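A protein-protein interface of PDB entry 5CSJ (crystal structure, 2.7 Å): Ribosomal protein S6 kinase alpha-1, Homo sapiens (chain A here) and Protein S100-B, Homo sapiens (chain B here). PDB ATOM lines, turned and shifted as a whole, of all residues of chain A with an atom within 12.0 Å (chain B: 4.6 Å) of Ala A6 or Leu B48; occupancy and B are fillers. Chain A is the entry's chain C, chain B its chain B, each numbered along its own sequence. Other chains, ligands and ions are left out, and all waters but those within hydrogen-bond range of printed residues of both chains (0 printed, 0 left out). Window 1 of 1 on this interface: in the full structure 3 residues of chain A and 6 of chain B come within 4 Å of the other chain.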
ATOM      1  N   GLY A   3      17.391  -6.907  24.421  1.00  0.00           N
ATOM      2  CA  GLY A   3      16.334  -5.915  24.297  1.00  0.00           C
ATOM      3  C   GLY A   3      14.964  -6.506  23.988  1.00  0.00           C
ATOM      4  O   GLY A   3      14.505  -6.426  22.843  1.00  0.00           O
ATOM      5  N   ALA A   4      14.314  -7.082  25.006  1.00  0.00           N
ATOM      6  CA  ALA A   4      12.980  -7.687  24.866  1.00  0.00           C
ATOM      7  C   ALA A   4      11.881  -6.670  25.131  1.00  0.00           C
ATOM      8  O   ALA A   4      11.449  -6.506  26.273  1.00  0.00           O
ATOM      9  CB  ALA A   4      12.825  -8.880  25.822  1.00  0.00           C
ATOM     10  N   MET A   5      11.421  -5.997  24.079  1.00  0.00           N
ATOM     11  CA  MET A   5      10.432  -4.935  24.240  1.00  0.00           C
ATOM     12  C   MET A   5       9.178  -5.143  23.388  1.00  0.00           C
ATOM     13  O   MET A   5       9.235  -5.698  22.283  1.00  0.00           O
ATOM     14  CB  MET A   5      11.063  -3.579  23.909  1.00  0.00           C
ATOM     15  CG  MET A   5      12.285  -3.240  24.743  1.00  0.00           C
ATOM     16  SD  MET A   5      13.734  -2.925  23.714  1.00  0.00           S
ATOM     17  CE  MET A   5      14.970  -2.522  24.956  1.00  0.00           C
ATOM     18  N   ALA A   6       8.043  -4.692  23.916  1.00  0.00           N
ATOM     19  CA  ALA A   6       6.793  -4.712  23.164  1.00  0.00           C
ATOM     20  C   ALA A   6       6.577  -3.363  22.458  1.00  0.00           C
ATOM     21  O   ALA A   6       7.116  -2.334  22.880  1.00  0.00           O
ATOM     22  CB  ALA A   6       5.610  -5.055  24.091  1.00  0.00           C
ATOM     23  N   ALA A   7       5.791  -3.377  21.382  1.00  0.00           N
ATOM     24  CA  ALA A   7       5.564  -2.179  20.574  1.00  0.00           C
ATOM     25  C   ALA A   7       4.462  -1.271  21.149  1.00  0.00           C
ATOM     26  O   ALA A   7       3.752  -0.584  20.396  1.00  0.00           O
ATOM     27  CB  ALA A   7       5.225  -2.580  19.135  1.00  0.00           C
ATOM     28  N   THR A   8       4.323  -1.271  22.480  1.00  0.00           N
ATOM     29  CA  THR A   8       3.412  -0.367  23.217  1.00  0.00           C
ATOM     30  C   THR A   8       1.925  -0.433  22.822  1.00  0.00           C
ATOM     31  O   THR A   8       1.120   0.330  23.362  1.00  0.00           O
ATOM     32  CB  THR A   8       3.863   1.140  23.101  1.00  0.00           C
ATOM     33  OG1 THR A   8       3.819   1.563  21.733  1.00  0.00           O
ATOM     34  CG2 THR A   8       5.264   1.372  23.672  1.00  0.00           C
ATOM     35  N   TYR A   9       1.550  -1.335  21.912  1.00  0.00           N
ATOM     36  CA  TYR A   9       0.140  -1.547  21.551  1.00  0.00           C
ATOM     37  C   TYR A   9      -0.544  -2.566  22.485  1.00  0.00           C
ATOM     38  O   TYR A   9      -1.696  -2.964  22.258  1.00  0.00           O
ATOM     39  CB  TYR A   9       0.030  -2.028  20.095  1.00  0.00           C
ATOM     40  N   SER A  10       0.164  -2.968  23.538  1.00  0.00           N
ATOM     41  CA  SER A  10      -0.332  -3.938  24.509  1.00  0.00           C
ATOM     42  C   SER A  10      -0.284  -3.377  25.923  1.00  0.00           C
ATOM     43  O   SER A  10       0.736  -3.481  26.605  1.00  0.00           O
ATOM     44  CB  SER A  10       0.494  -5.226  24.436  1.00  0.00           C
ATOM     45  OG  SER A  10       0.564  -5.712  23.109  1.00  0.00           O
ATOM     46  N   ILE B  40       7.506   7.546  28.836  1.00  0.00           N
ATOM     47  CA  ILE B  40       7.726   6.220  28.278  1.00  0.00           C
ATOM     48  C   ILE B  40       9.176   6.137  27.752  1.00  0.00           C
ATOM     49  O   ILE B  40       9.854   5.133  27.957  1.00  0.00           O
ATOM     50  CB  ILE B  40       6.703   5.910  27.177  1.00  0.00           C
ATOM     51  CG1 ILE B  40       5.325   5.717  27.810  1.00  0.00           C
ATOM     52  CG2 ILE B  40       7.082   4.676  26.426  1.00  0.00           C
ATOM     53  CD1 ILE B  40       4.218   5.574  26.845  1.00  0.00           C
ATOM     54  N   LEU B  44      10.734   4.074  30.741  1.00  0.00           N
ATOM     55  CA  LEU B  44      10.310   2.705  30.468  1.00  0.00           C
ATOM     56  C   LEU B  44      11.071   2.127  29.303  1.00  0.00           C
ATOM     57  O   LEU B  44      10.592   1.201  28.648  1.00  0.00           O
ATOM     58  CB  LEU B  44       8.819   2.636  30.166  1.00  0.00           C
ATOM     59  CG  LEU B  44       7.896   2.805  31.362  1.00  0.00           C
ATOM     60  CD1 LEU B  44       6.516   2.849  30.861  1.00  0.00           C
ATOM     61  CD2 LEU B  44       8.118   1.644  32.288  1.00  0.00           C
ATOM     62  N   SER B  45      12.283   2.642  29.102  1.00  0.00           N
ATOM     63  CA  SER B  45      13.110   2.326  27.936  1.00  0.00           C
ATOM     64  C   SER B  45      13.611   0.893  27.854  1.00  0.00           C
ATOM     65  O   SER B  45      13.924   0.418  26.772  1.00  0.00           O
ATOM     66  CB  SER B  45      14.289   3.284  27.876  1.00  0.00           C
ATOM     67  OG  SER B  45      15.135   3.087  28.976  1.00  0.00           O
ATOM     68  N   HIS B  46      13.642   0.187  28.970  1.00  0.00           N
ATOM     69  CA  HIS B  46      14.073  -1.208  28.933  1.00  0.00           C
ATOM     70  C   HIS B  46      12.900  -2.170  28.739  1.00  0.00           C
ATOM     71  O   HIS B  46      13.111  -3.336  28.478  1.00  0.00           O
ATOM     72  CB  HIS B  46      14.862  -1.591  30.205  1.00  0.00           C
ATOM     73  CG  HIS B  46      15.992  -0.661  30.501  1.00  0.00           C
ATOM     74  ND1 HIS B  46      15.866   0.429  31.336  1.00  0.00           N
ATOM     75  CD2 HIS B  46      17.242  -0.590  29.984  1.00  0.00           C
ATOM     76  CE1 HIS B  46      17.008   1.094  31.373  1.00  0.00           C
ATOM     77  NE2 HIS B  46      17.861   0.498  30.557  1.00  0.00           N
ATOM     78  N   PHE B  47      11.670  -1.680  28.832  1.00  0.00           N
ATOM     79  CA  PHE B  47      10.480  -2.533  28.707  1.00  0.00           C
ATOM     80  C   PHE B  47       9.697  -2.237  27.429  1.00  0.00           C
ATOM     81  O   PHE B  47       9.224  -3.138  26.737  1.00  0.00           O
ATOM     82  CB  PHE B  47       9.552  -2.339  29.909  1.00  0.00           C
ATOM     83  CG  PHE B  47      10.130  -2.798  31.229  1.00  0.00           C
ATOM     84  CD1 PHE B  47      11.257  -3.625  31.282  1.00  0.00           C
ATOM     85  CD2 PHE B  47       9.553  -2.380  32.426  1.00  0.00           C
ATOM     86  CE1 PHE B  47      11.792  -4.033  32.505  1.00  0.00           C
ATOM     87  CE2 PHE B  47      10.087  -2.775  33.652  1.00  0.00           C
ATOM     88  CZ  PHE B  47      11.200  -3.603  33.692  1.00  0.00           C
ATOM     89  N   LEU B  48       9.588  -0.961  27.105  1.00  0.00           N
ATOM     90  CA  LEU B  48       8.903  -0.565  25.897  1.00  0.00           C
ATOM     91  C   LEU B  48       9.859  -0.041  24.856  1.00  0.00           C
ATOM     92  O   LEU B  48      10.902   0.525  25.168  1.00  0.00           O
ATOM     93  CB  LEU B  48       7.835   0.480  26.189  1.00  0.00           C
ATOM     94  CG  LEU B  48       6.823   0.026  27.204  1.00  0.00           C
ATOM     95  CD1 LEU B  48       5.800   1.089  27.421  1.00  0.00           C
ATOM     96  CD2 LEU B  48       6.194  -1.143  26.535  1.00  0.00           C
ATOM     97  N   GLU B  49       9.509  -0.348  23.613  1.00  0.00           N
ATOM     98  CA  GLU B  49      10.187   0.149  22.447  1.00  0.00           C
ATOM     99  C   GLU B  49      10.017   1.652  22.444  1.00  0.00           C
ATOM    100  O   GLU B  49       9.013   2.157  22.939  1.00  0.00           O
ATOM    101  CB  GLU B  49       9.582  -0.498  21.208  1.00  0.00           C
ATOM    102  CG  GLU B  49      10.504  -0.647  20.027  1.00  0.00           C
ATOM    103  CD  GLU B  49      10.191  -1.899  19.209  1.00  0.00           C
ATOM    104  OE1 GLU B  49      10.560  -1.932  18.015  1.00  0.00           O
ATOM    105  OE2 GLU B  49       9.582  -2.849  19.757  1.00  0.00           O
ATOM    106  N   GLU B  50      11.035   2.375  21.994  1.00  0.00           N
ATOM    107  CA  GLU B  50      10.952   3.831  21.976  1.00  0.00           C
ATOM    108  C   GLU B  50       9.745   4.309  21.182  1.00  0.00           C
ATOM    109  O   GLU B  50       9.460   3.767  20.121  1.00  0.00           O
ATOM    110  CB  GLU B  50      12.205   4.426  21.350  1.00  0.00           C
ATOM    111  CG  GLU B  50      12.241   5.919  21.393  1.00  0.00           C
ATOM    112  CD  GLU B  50      13.547   6.467  20.890  1.00  0.00           C
ATOM    113  OE1 GLU B  50      14.310   5.690  20.260  1.00  0.00           O
ATOM    114  OE2 GLU B  50      13.808   7.672  21.125  1.00  0.00           O
ATOM    115  N   PHE B  80      -2.224   2.160  33.313  1.00  0.00           N
ATOM    116  CA  PHE B  80      -1.096   2.019  32.402  1.00  0.00           C
ATOM    117  C   PHE B  80      -0.003   1.155  33.055  1.00  0.00           C
ATOM    118  O   PHE B  80       0.518   0.229  32.427  1.00  0.00           O
ATOM    119  CB  PHE B  80      -0.552   3.381  32.019  1.00  0.00           C
ATOM    120  CG  PHE B  80       0.631   3.330  31.128  1.00  0.00           C
ATOM    121  CD1 PHE B  80       0.538   2.782  29.863  1.00  0.00           C
ATOM    122  CD2 PHE B  80       1.841   3.869  31.539  1.00  0.00           C
ATOM    123  CE1 PHE B  80       1.640   2.749  29.041  1.00  0.00           C
ATOM    124  CE2 PHE B  80       2.937   3.827  30.723  1.00  0.00           C
ATOM    125  CZ  PHE B  80       2.834   3.261  29.476  1.00  0.00           C
ATOM    126  N   VAL B  84       1.217  -2.544  31.538  1.00  0.00           N
ATOM    127  CA  VAL B  84       2.608  -2.754  31.210  1.00  0.00           C
ATOM    128  C   VAL B  84       3.209  -3.807  32.113  1.00  0.00           C
ATOM    129  O   VAL B  84       3.841  -4.732  31.621  1.00  0.00           O
ATOM    130  CB  VAL B  84       3.438  -1.453  31.327  1.00  0.00           C
ATOM    131  CG1 VAL B  84       4.899  -1.711  30.986  1.00  0.00           C
ATOM    132  CG2 VAL B  84       2.846  -0.358  30.489  1.00  0.00           C
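O of Phe B47 sits at hydrogen-bond distance from N of Ala A6, at 3.4 Å.
N of Glu B49 lies within hydrogen-bond range of O of Ala A6 (3.2 Å).
Among the printed residues, pairs that only touch across the chains: Met A5 with Ser B45 (3.6 Å), Met A5 with His B46 (3.8 Å), Met A5 with Phe B47 (3.3 Å), Met A5 with Leu B48 (3.9 Å), Met A5 with Glu B49 (3.6 Å), Ala A6 with Leu B48 (3.9 Å), Thr A8 with Leu B48 (3.7 Å) and Thr A8 with Glu B49 (3.9 Å).
Ala A6 touches three residues of chain B.
Of chain A, only Met A5 (3.9 Å), Ala A6 (3.9 Å) and Thr A8 (3.7 Å) come within 4 Å of Leu B48.
No residue of chain A comes within 4 Å of Ile B40.
No residue of chain A comes within 4 Å of Leu B44.
Of the printed residues of chain A, Phe B47 touches Met A5 and Ala A6.
No residue of chain A comes within 4 Å of Val B84.
Printed residues of chain B within 4 Å of Met A5: Ser B45 (3.6 Å), His B46 (3.8 Å), Phe B47 (3.3 Å), Leu B48 (3.9 Å) and Glu B49 (3.6 Å).
Of the printed residues of chain B, Thr A8 touches Leu B48 (3.7 Å) and Glu B49 (3.9 Å).
Printed residues of chain A within 4 Å of His B46: Met A5.
Gly A3 touches none of the printed residues of chain B.
Of the 8 printed residues of chain A, 3 touch a printed residue of chain B.
Hydrophobic or aromatic side chains of chain A within 4 Å of the printed part of chain B: Met A5.
Hydrophobic or aromatic side chains of chain B that line the printed part of chain A: Leu B48.
Among the printed residues, 10 pairs touch across the chains.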
